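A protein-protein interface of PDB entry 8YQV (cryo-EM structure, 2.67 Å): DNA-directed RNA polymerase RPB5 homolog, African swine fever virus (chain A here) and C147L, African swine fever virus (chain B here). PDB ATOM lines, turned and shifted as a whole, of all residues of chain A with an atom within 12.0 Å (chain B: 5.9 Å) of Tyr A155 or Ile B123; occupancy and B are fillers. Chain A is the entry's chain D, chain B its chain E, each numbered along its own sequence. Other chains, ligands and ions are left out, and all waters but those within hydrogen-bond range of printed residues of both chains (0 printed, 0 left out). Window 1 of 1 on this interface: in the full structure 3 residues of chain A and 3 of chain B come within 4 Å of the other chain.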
ATOM      1  N   GLU A 146     -11.573 -18.613   1.593  1.00  0.00           N
ATOM      2  CA  GLU A 146     -11.991 -17.229   1.783  1.00  0.00           C
ATOM      3  C   GLU A 146     -10.802 -16.285   1.725  1.00  0.00           C
ATOM      4  O   GLU A 146     -10.881 -15.210   1.119  1.00  0.00           O
ATOM      5  CB  GLU A 146     -12.734 -17.086   3.109  1.00  0.00           C
ATOM      6  CG  GLU A 146     -14.084 -17.773   3.129  1.00  0.00           C
ATOM      7  CD  GLU A 146     -14.756 -17.716   4.487  1.00  0.00           C
ATOM      8  OE1 GLU A 146     -14.102 -17.294   5.463  1.00  0.00           O
ATOM      9  OE2 GLU A 146     -15.942 -18.095   4.579  1.00  0.00           O
ATOM     10  N   ALA A 147      -9.686 -16.674   2.336  1.00  0.00           N
ATOM     11  CA  ALA A 147      -8.480 -15.862   2.252  1.00  0.00           C
ATOM     12  C   ALA A 147      -7.970 -15.774   0.823  1.00  0.00           C
ATOM     13  O   ALA A 147      -7.505 -14.716   0.393  1.00  0.00           O
ATOM     14  CB  ALA A 147      -7.400 -16.430   3.160  1.00  0.00           C
ATOM     15  N   GLN A 148      -8.031 -16.875   0.072  1.00  0.00           N
ATOM     16  CA  GLN A 148      -7.567 -16.829  -1.307  1.00  0.00           C
ATOM     17  C   GLN A 148      -8.424 -15.905  -2.151  1.00  0.00           C
ATOM     18  O   GLN A 148      -7.888 -15.160  -2.974  1.00  0.00           O
ATOM     19  CB  GLN A 148      -7.535 -18.226  -1.926  1.00  0.00           C
ATOM     20  CG  GLN A 148      -6.397 -19.104  -1.427  1.00  0.00           C
ATOM     21  CD  GLN A 148      -5.051 -18.412  -1.461  1.00  0.00           C
ATOM     22  OE1 GLN A 148      -4.706 -17.744  -2.434  1.00  0.00           O
ATOM     23  NE2 GLN A 148      -4.286 -18.562  -0.387  1.00  0.00           N
ATOM     24  N   GLU A 149      -9.744 -15.923  -1.967  1.00  0.00           N
ATOM     25  CA  GLU A 149     -10.569 -15.011  -2.753  1.00  0.00           C
ATOM     26  C   GLU A 149     -10.364 -13.562  -2.321  1.00  0.00           C
ATOM     27  O   GLU A 149     -10.362 -12.662  -3.170  1.00  0.00           O
ATOM     28  CB  GLU A 149     -12.042 -15.414  -2.682  1.00  0.00           C
ATOM     29  CG  GLU A 149     -12.776 -15.029  -1.425  1.00  0.00           C
ATOM     30  CD  GLU A 149     -14.170 -15.619  -1.371  1.00  0.00           C
ATOM     31  OE1 GLU A 149     -14.505 -16.434  -2.256  1.00  0.00           O
ATOM     32  OE2 GLU A 149     -14.935 -15.266  -0.449  1.00  0.00           O
ATOM     33  N   PHE A 150     -10.150 -13.319  -1.026  1.00  0.00           N
ATOM     34  CA  PHE A 150      -9.838 -11.969  -0.564  1.00  0.00           C
ATOM     35  C   PHE A 150      -8.553 -11.460  -1.199  1.00  0.00           C
ATOM     36  O   PHE A 150      -8.501 -10.339  -1.717  1.00  0.00           O
ATOM     37  CB  PHE A 150      -9.727 -11.964   0.962  1.00  0.00           C
ATOM     38  CG  PHE A 150      -9.134 -10.706   1.528  1.00  0.00           C
ATOM     39  CD1 PHE A 150      -9.889  -9.558   1.639  1.00  0.00           C
ATOM     40  CD2 PHE A 150      -7.823 -10.678   1.957  1.00  0.00           C
ATOM     41  CE1 PHE A 150      -9.345  -8.412   2.158  1.00  0.00           C
ATOM     42  CE2 PHE A 150      -7.280  -9.532   2.472  1.00  0.00           C
ATOM     43  CZ  PHE A 150      -8.041  -8.400   2.573  1.00  0.00           C
ATOM     44  N   LEU A 151      -7.507 -12.286  -1.185  1.00  0.00           N
ATOM     45  CA  LEU A 151      -6.222 -11.881  -1.739  1.00  0.00           C
ATOM     46  C   LEU A 151      -6.284 -11.731  -3.250  1.00  0.00           C
ATOM     47  O   LEU A 151      -5.615 -10.860  -3.811  1.00  0.00           O
ATOM     48  CB  LEU A 151      -5.148 -12.892  -1.350  1.00  0.00           C
ATOM     49  CG  LEU A 151      -4.810 -13.036   0.131  1.00  0.00           C
ATOM     50  CD1 LEU A 151      -4.044 -14.313   0.355  1.00  0.00           C
ATOM     51  CD2 LEU A 151      -4.013 -11.859   0.623  1.00  0.00           C
ATOM     52  N   GLY A 152      -7.065 -12.571  -3.927  1.00  0.00           N
ATOM     53  CA  GLY A 152      -7.228 -12.420  -5.358  1.00  0.00           C
ATOM     54  C   GLY A 152      -7.949 -11.148  -5.739  1.00  0.00           C
ATOM     55  O   GLY A 152      -7.595 -10.505  -6.731  1.00  0.00           O
ATOM     56  N   ARG A 153      -8.970 -10.766  -4.973  1.00  0.00           N
ATOM     57  CA  ARG A 153      -9.613  -9.479  -5.208  1.00  0.00           C
ATOM     58  C   ARG A 153      -8.657  -8.329  -4.919  1.00  0.00           C
ATOM     59  O   ARG A 153      -8.676  -7.310  -5.615  1.00  0.00           O
ATOM     60  CB  ARG A 153     -10.876  -9.364  -4.361  1.00  0.00           C
ATOM     61  CG  ARG A 153     -11.782  -8.207  -4.722  1.00  0.00           C
ATOM     62  CD  ARG A 153     -11.644  -7.059  -3.749  1.00  0.00           C
ATOM     63  NE  ARG A 153     -12.451  -5.919  -4.159  1.00  0.00           N
ATOM     64  CZ  ARG A 153     -12.280  -4.682  -3.721  1.00  0.00           C
ATOM     65  NH1 ARG A 153     -11.345  -4.387  -2.837  1.00  0.00           N
ATOM     66  NH2 ARG A 153     -13.066  -3.717  -4.183  1.00  0.00           N
ATOM     67  N   GLU A 154      -7.813  -8.474  -3.905  1.00  0.00           N
ATOM     68  CA  GLU A 154      -6.913  -7.409  -3.493  1.00  0.00           C
ATOM     69  C   GLU A 154      -5.580  -7.415  -4.227  1.00  0.00           C
ATOM     70  O   GLU A 154      -4.783  -6.497  -4.019  1.00  0.00           O
ATOM     71  CB  GLU A 154      -6.661  -7.500  -1.988  1.00  0.00           C
ATOM     72  CG  GLU A 154      -7.891  -7.261  -1.147  1.00  0.00           C
ATOM     73  CD  GLU A 154      -8.191  -5.802  -0.960  1.00  0.00           C
ATOM     74  OE1 GLU A 154      -7.252  -5.040  -0.669  1.00  0.00           O
ATOM     75  OE2 GLU A 154      -9.362  -5.410  -1.111  1.00  0.00           O
ATOM     76  N   TYR A 155      -5.320  -8.409  -5.075  1.00  0.00           N
ATOM     77  CA  TYR A 155      -4.038  -8.559  -5.764  1.00  0.00           C
ATOM     78  C   TYR A 155      -2.882  -8.575  -4.772  1.00  0.00           C
ATOM     79  O   TYR A 155      -1.863  -7.911  -4.953  1.00  0.00           O
ATOM     80  CB  TYR A 155      -3.832  -7.463  -6.810  1.00  0.00           C
ATOM     81  CG  TYR A 155      -4.578  -7.686  -8.097  1.00  0.00           C
ATOM     82  CD1 TYR A 155      -4.097  -8.557  -9.057  1.00  0.00           C
ATOM     83  CD2 TYR A 155      -5.758  -7.019  -8.354  1.00  0.00           C
ATOM     84  CE1 TYR A 155      -4.779  -8.760 -10.229  1.00  0.00           C
ATOM     85  CE2 TYR A 155      -6.445  -7.216  -9.520  1.00  0.00           C
ATOM     86  CZ  TYR A 155      -5.953  -8.085 -10.456  1.00  0.00           C
ATOM     87  OH  TYR A 155      -6.641  -8.277 -11.624  1.00  0.00           O
ATOM     88  N   LEU A 156      -3.049  -9.349  -3.708  1.00  0.00           N
ATOM     89  CA  LEU A 156      -2.077  -9.418  -2.632  1.00  0.00           C
ATOM     90  C   LEU A 156      -1.517 -10.826  -2.524  1.00  0.00           C
ATOM     91  O   LEU A 156      -2.186 -11.809  -2.850  1.00  0.00           O
ATOM     92  CB  LEU A 156      -2.697  -9.019  -1.293  1.00  0.00           C
ATOM     93  CG  LEU A 156      -3.002  -7.554  -1.009  1.00  0.00           C
ATOM     94  CD1 LEU A 156      -3.783  -7.437   0.268  1.00  0.00           C
ATOM     95  CD2 LEU A 156      -1.732  -6.752  -0.912  1.00  0.00           C
ATOM     96  N   GLN A 157      -0.289 -10.909  -2.085  1.00  0.00           N
ATOM     97  CA  GLN A 157       0.310 -12.150  -1.642  1.00  0.00           C
ATOM     98  C   GLN A 157       0.219 -12.243  -0.131  1.00  0.00           C
ATOM     99  O   GLN A 157       0.165 -11.223   0.559  1.00  0.00           O
ATOM    100  CB  GLN A 157       1.776 -12.226  -2.081  1.00  0.00           C
ATOM    101  CG  GLN A 157       2.001 -12.027  -3.564  1.00  0.00           C
ATOM    102  CD  GLN A 157       1.281 -13.056  -4.405  1.00  0.00           C
ATOM    103  OE1 GLN A 157       1.224 -14.232  -4.056  1.00  0.00           O
ATOM    104  NE2 GLN A 157       0.724 -12.617  -5.524  1.00  0.00           N
ATOM    105  N   PRO A 158       0.197 -13.454   0.431  1.00  0.00           N
ATOM    106  CA  PRO A 158       0.083 -13.579   1.891  1.00  0.00           C
ATOM    107  C   PRO A 158       1.191 -12.885   2.654  1.00  0.00           C
ATOM    108  O   PRO A 158       1.003 -12.581   3.835  1.00  0.00           O
ATOM    109  CB  PRO A 158       0.119 -15.094   2.112  1.00  0.00           C
ATOM    110  CG  PRO A 158      -0.394 -15.657   0.853  1.00  0.00           C
ATOM    111  CD  PRO A 158       0.117 -14.763  -0.233  1.00  0.00           C
ATOM    112  N   GLN A 159       2.331 -12.623   2.026  1.00  0.00           N
ATOM    113  CA  GLN A 159       3.423 -11.906   2.665  1.00  0.00           C
ATOM    114  C   GLN A 159       3.213 -10.401   2.691  1.00  0.00           C
ATOM    115  O   GLN A 159       3.934  -9.704   3.410  1.00  0.00           O
ATOM    116  CB  GLN A 159       4.736 -12.217   1.953  1.00  0.00           C
ATOM    117  CG  GLN A 159       5.337 -13.554   2.316  1.00  0.00           C
ATOM    118  CD  GLN A 159       4.545 -14.718   1.768  1.00  0.00           C
ATOM    119  OE1 GLN A 159       4.176 -15.632   2.502  1.00  0.00           O
ATOM    120  NE2 GLN A 159       4.272 -14.688   0.471  1.00  0.00           N
ATOM    121  N   ASP A 160       2.255  -9.884   1.924  1.00  0.00           N
ATOM    122  CA  ASP A 160       1.958  -8.461   1.930  1.00  0.00           C
ATOM    123  C   ASP A 160       1.065  -8.044   3.087  1.00  0.00           C
ATOM    124  O   ASP A 160       0.980  -6.849   3.375  1.00  0.00           O
ATOM    125  CB  ASP A 160       1.295  -8.058   0.614  1.00  0.00           C
ATOM    126  CG  ASP A 160       2.150  -8.374  -0.593  1.00  0.00           C
ATOM    127  OD1 ASP A 160       3.387  -8.251  -0.502  1.00  0.00           O
ATOM    128  OD2 ASP A 160       1.586  -8.726  -1.647  1.00  0.00           O
ATOM    129  N   LEU A 161       0.412  -8.986   3.757  1.00  0.00           N
ATOM    130  CA  LEU A 161      -0.471  -8.674   4.864  1.00  0.00           C
ATOM    131  C   LEU A 161       0.330  -8.329   6.113  1.00  0.00           C
ATOM    132  O   LEU A 161       1.517  -8.631   6.222  1.00  0.00           O
ATOM    133  CB  LEU A 161      -1.390  -9.852   5.165  1.00  0.00           C
ATOM    134  CG  LEU A 161      -2.357 -10.326   4.094  1.00  0.00           C
ATOM    135  CD1 LEU A 161      -3.109 -11.529   4.602  1.00  0.00           C
ATOM    136  CD2 LEU A 161      -3.311  -9.223   3.714  1.00  0.00           C
ATOM    137  N   PHE A 181      -4.879 -17.639   8.175  1.00  0.00           N
ATOM    138  CA  PHE A 181      -5.264 -16.240   8.220  1.00  0.00           C
ATOM    139  C   PHE A 181      -6.291 -16.027   9.318  1.00  0.00           C
ATOM    140  O   PHE A 181      -7.251 -16.798   9.451  1.00  0.00           O
ATOM    141  CB  PHE A 181      -5.830 -15.764   6.878  1.00  0.00           C
ATOM    142  CG  PHE A 181      -4.944 -16.048   5.701  1.00  0.00           C
ATOM    143  CD1 PHE A 181      -4.862 -17.316   5.160  1.00  0.00           C
ATOM    144  CD2 PHE A 181      -4.196 -15.041   5.134  1.00  0.00           C
ATOM    145  CE1 PHE A 181      -4.058 -17.566   4.084  1.00  0.00           C
ATOM    146  CE2 PHE A 181      -3.390 -15.291   4.060  1.00  0.00           C
ATOM    147  CZ  PHE A 181      -3.320 -16.556   3.535  1.00  0.00           C
ATOM    148  N   ILE A 197      -7.231  -8.485   8.250  1.00  0.00           N
ATOM    149  CA  ILE A 197      -6.864  -9.886   8.115  1.00  0.00           C
ATOM    150  C   ILE A 197      -5.357  -9.983   8.267  1.00  0.00           C
ATOM    151  O   ILE A 197      -4.614  -9.281   7.573  1.00  0.00           O
ATOM    152  CB  ILE A 197      -7.330 -10.480   6.778  1.00  0.00           C
ATOM    153  CG1 ILE A 197      -8.845 -10.648   6.800  1.00  0.00           C
ATOM    154  CG2 ILE A 197      -6.680 -11.809   6.537  1.00  0.00           C
ATOM    155  CD1 ILE A 197      -9.420 -11.225   5.555  1.00  0.00           C
ATOM    156  N   ILE B  60      -6.788  -4.489 -17.354  1.00  0.00           N
ATOM    157  CA  ILE B  60      -8.017  -5.006 -16.749  1.00  0.00           C
ATOM    158  C   ILE B  60      -9.210  -4.561 -17.584  1.00  0.00           C
ATOM    159  O   ILE B  60      -9.327  -3.363 -17.904  1.00  0.00           O
ATOM    160  CB  ILE B  60      -8.153  -4.511 -15.301  1.00  0.00           C
ATOM    161  CG1 ILE B  60      -7.004  -5.034 -14.451  1.00  0.00           C
ATOM    162  CG2 ILE B  60      -9.456  -4.966 -14.708  1.00  0.00           C
ATOM    163  CD1 ILE B  60      -7.012  -4.507 -13.049  1.00  0.00           C
ATOM    164  N   ILE B  66     -11.642  -1.633 -10.352  1.00  0.00           N
ATOM    165  CA  ILE B  66     -11.990  -1.452  -8.955  1.00  0.00           C
ATOM    166  C   ILE B  66     -11.758  -0.025  -8.468  1.00  0.00           C
ATOM    167  O   ILE B  66     -12.451   0.422  -7.549  1.00  0.00           O
ATOM    168  CB  ILE B  66     -11.208  -2.470  -8.095  1.00  0.00           C
ATOM    169  CG1 ILE B  66     -11.661  -3.888  -8.411  1.00  0.00           C
ATOM    170  CG2 ILE B  66     -11.303  -2.184  -6.620  1.00  0.00           C
ATOM    171  CD1 ILE B  66     -10.769  -4.945  -7.812  1.00  0.00           C
ATOM    172  N   THR B  67     -10.834   0.713  -9.074  1.00  0.00           N
ATOM    173  CA  THR B  67     -10.520   2.058  -8.628  1.00  0.00           C
ATOM    174  C   THR B  67     -11.662   3.017  -8.950  1.00  0.00           C
ATOM    175  O   THR B  67     -12.596   2.695  -9.685  1.00  0.00           O
ATOM    176  CB  THR B  67      -9.219   2.533  -9.264  1.00  0.00           C
ATOM    177  OG1 THR B  67      -9.265   2.289 -10.672  1.00  0.00           O
ATOM    178  CG2 THR B  67      -8.055   1.795  -8.682  1.00  0.00           C
ATOM    179  N   ARG B 121      -3.348   3.358 -14.152  1.00  0.00           N
ATOM    180  CA  ARG B 121      -3.213   3.051 -12.735  1.00  0.00           C
ATOM    181  C   ARG B 121      -2.581   1.673 -12.612  1.00  0.00           C
ATOM    182  O   ARG B 121      -3.228   0.662 -12.894  1.00  0.00           O
ATOM    183  CB  ARG B 121      -4.571   3.115 -12.041  1.00  0.00           C
ATOM    184  CG  ARG B 121      -5.078   4.526 -11.822  1.00  0.00           C
ATOM    185  CD  ARG B 121      -6.507   4.561 -11.339  1.00  0.00           C
ATOM    186  NE  ARG B 121      -6.924   5.906 -10.966  1.00  0.00           N
ATOM    187  CZ  ARG B 121      -8.183   6.297 -10.840  1.00  0.00           C
ATOM    188  NH1 ARG B 121      -9.187   5.468 -11.048  1.00  0.00           N
ATOM    189  NH2 ARG B 121      -8.440   7.554 -10.499  1.00  0.00           N
ATOM    190  N   CYS B 122      -1.317   1.630 -12.201  1.00  0.00           N
ATOM    191  CA  CYS B 122      -0.565   0.382 -12.138  1.00  0.00           C
ATOM    192  C   CYS B 122      -0.980  -0.397 -10.899  1.00  0.00           C
ATOM    193  O   CYS B 122      -0.617  -0.033  -9.778  1.00  0.00           O
ATOM    194  CB  CYS B 122       0.933   0.664 -12.124  1.00  0.00           C
ATOM    195  SG  CYS B 122       1.527   1.610 -13.530  1.00  0.00           S
ATOM    196  N   ILE B 123      -1.716  -1.486 -11.104  1.00  0.00           N
ATOM    197  CA  ILE B 123      -2.245  -2.252  -9.983  1.00  0.00           C
ATOM    198  C   ILE B 123      -1.201  -3.216  -9.440  1.00  0.00           C
ATOM    199  O   ILE B 123      -0.926  -3.233  -8.236  1.00  0.00           O
ATOM    200  CB  ILE B 123      -3.530  -2.985 -10.397  1.00  0.00           C
ATOM    201  CG1 ILE B 123      -4.591  -1.976 -10.824  1.00  0.00           C
ATOM    202  CG2 ILE B 123      -4.032  -3.842  -9.265  1.00  0.00           C
ATOM    203  CD1 ILE B 123      -4.890  -0.944  -9.780  1.00  0.00           C
ATOM    204  N   LYS B 124      -0.600  -4.034 -10.301  1.00  0.00           N
ATOM    205  CA  LYS B 124       0.360  -5.002  -9.786  1.00  0.00           C
ATOM    206  C   LYS B 124       1.404  -5.361 -10.834  1.00  0.00           C
ATOM    207  O   LYS B 124       1.161  -5.229 -12.030  1.00  0.00           O
ATOM    208  CB  LYS B 124      -0.341  -6.277  -9.307  1.00  0.00           C
ATOM    209  CG  LYS B 124       0.573  -7.193  -8.533  1.00  0.00           C
ATOM    210  CD  LYS B 124      -0.080  -8.476  -8.137  1.00  0.00           C
ATOM    211  CE  LYS B 124       0.940  -9.360  -7.472  1.00  0.00           C
ATOM    212  NZ  LYS B 124       1.573  -8.646  -6.334  1.00  0.00           N
ATOM    213  N   VAL B 125       2.568  -5.803 -10.372  1.00  0.00           N
ATOM    214  CA  VAL B 125       3.586  -6.405 -11.224  1.00  0.00           C
ATOM    215  C   VAL B 125       3.778  -7.845 -10.765  1.00  0.00           C
ATOM    216  O   VAL B 125       4.423  -8.103  -9.745  1.00  0.00           O
ATOM    217  CB  VAL B 125       4.905  -5.625 -11.177  1.00  0.00           C
ATOM    218  CG1 VAL B 125       5.971  -6.365 -11.945  1.00  0.00           C
ATOM    219  CG2 VAL B 125       4.724  -4.241 -11.751  1.00  0.00           C
ATOM    220  N   ILE B 132      -0.212  -5.570 -14.493  1.00  0.00           N
ATOM    221  CA  ILE B 132      -1.659  -5.398 -14.496  1.00  0.00           C
ATOM    222  C   ILE B 132      -1.971  -3.950 -14.155  1.00  0.00           C
ATOM    223  O   ILE B 132      -1.585  -3.459 -13.087  1.00  0.00           O
ATOM    224  CB  ILE B 132      -2.330  -6.353 -13.501  1.00  0.00           C
ATOM    225  CG1 ILE B 132      -2.244  -7.791 -13.992  1.00  0.00           C
ATOM    226  CG2 ILE B 132      -3.764  -5.963 -13.272  1.00  0.00           C
ATOM    227  CD1 ILE B 132      -1.248  -8.606 -13.245  1.00  0.00           C
ATOM    228  N   VAL B 133      -2.673  -3.269 -15.065  1.00  0.00           N
ATOM    229  CA  VAL B 133      -2.980  -1.852 -14.953  1.00  0.00           C
ATOM    230  C   VAL B 133      -4.451  -1.642 -15.281  1.00  0.00           C
ATOM    231  O   VAL B 133      -5.113  -2.498 -15.861  1.00  0.00           O
ATOM    232  CB  VAL B 133      -2.106  -0.982 -15.880  1.00  0.00           C
ATOM    233  CG1 VAL B 133      -0.641  -1.192 -15.595  1.00  0.00           C
ATOM    234  CG2 VAL B 133      -2.420  -1.272 -17.333  1.00  0.00           C
ATOM    235  N   GLU B 134      -4.954  -0.474 -14.897  1.00  0.00           N
ATOM    236  CA  GLU B 134      -6.293  -0.026 -15.246  1.00  0.00           C
ATOM    237  C   GLU B 134      -6.183   1.249 -16.063  1.00  0.00           C
ATOM    238  O   GLU B 134      -5.515   2.196 -15.645  1.00  0.00           O
ATOM    239  CB  GLU B 134      -7.136   0.236 -14.003  1.00  0.00           C
ATOM    240  CG  GLU B 134      -7.948  -0.938 -13.543  1.00  0.00           C
ATOM    241  CD  GLU B 134      -8.345  -0.820 -12.098  1.00  0.00           C
ATOM    242  OE1 GLU B 134      -8.058   0.229 -11.498  1.00  0.00           O
ATOM    243  OE2 GLU B 134      -8.941  -1.769 -11.557  1.00  0.00           O
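N of Ile B123 is in hydrogen-bond range of O of Ile B132 (2.8 Å). N of Gln A157 is in hydrogen-bond range of OD2 of Asp A160. The backbone NH of Ile B132 sits at hydrogen-bond distance from the backbone carbonyl oxygen of Lys B124 (2.8 Å). The guanidinium group (NH1) of Arg A153 is in salt-bridge range of the side-chain carboxylate (OE2) of Glu A154 (2.8 Å). The side-chain carboxylate of Glu B134 lies within hydrogen-bond range of the backbone NH of Ile B66 (3.0 Å).
Among the printed residues, pairs that only touch across the chains: Arg A153 with Ile B66 (3.4 Å), Tyr A155 with Lys B124 (3.7 Å), Tyr A155 with Ile B123 (3.7 Å) and Gln A157 with Lys B124 (3.8 Å).
Of the printed residues of chain B, Arg A153 touches Ile B66 (3.4 Å). Of chain B, only Ile B123 and Lys B124 come within 4 Å of Tyr A155. Of the printed residues of chain B, Gln A157 touches Lys B124 (3.8 Å). Ile A197 touches none of the printed residues of chain B. Ile B60 touches none of the printed residues of chain A. Of the printed residues of chain A, Ile B66 touches Arg A153. Ile B123 touches just one residue of chain A: Tyr A155 (3.7 Å). Of chain A, only Tyr A155 (3.7 Å) and Gln A157 (3.8 Å) come within 4 Å of Lys B124. No residue of chain A comes within 4 Å of Ile B132. No residue of chain A comes within 4 Å of Val B133. The nearest printed residue of chain B that does not touch Arg A153 is Ile B123 (6.8 Å).
Of the 18 printed residues of chain A, 3 touch a printed residue of chain B. Hydrophobic or aromatic side chains of chain A within 4 Å of the printed part of chain B: Tyr A155. Of the 11 printed residues of chain B, 3 touch a printed residue of chain A. Printed residues of chain B that touch a printed residue of chain A: Ile B66, Ile B123 and Lys B124. Among the printed residues, no Asp or Glu carboxylate lies within 4 Å of a Lys or Arg side-chain nitrogen of the other chain.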
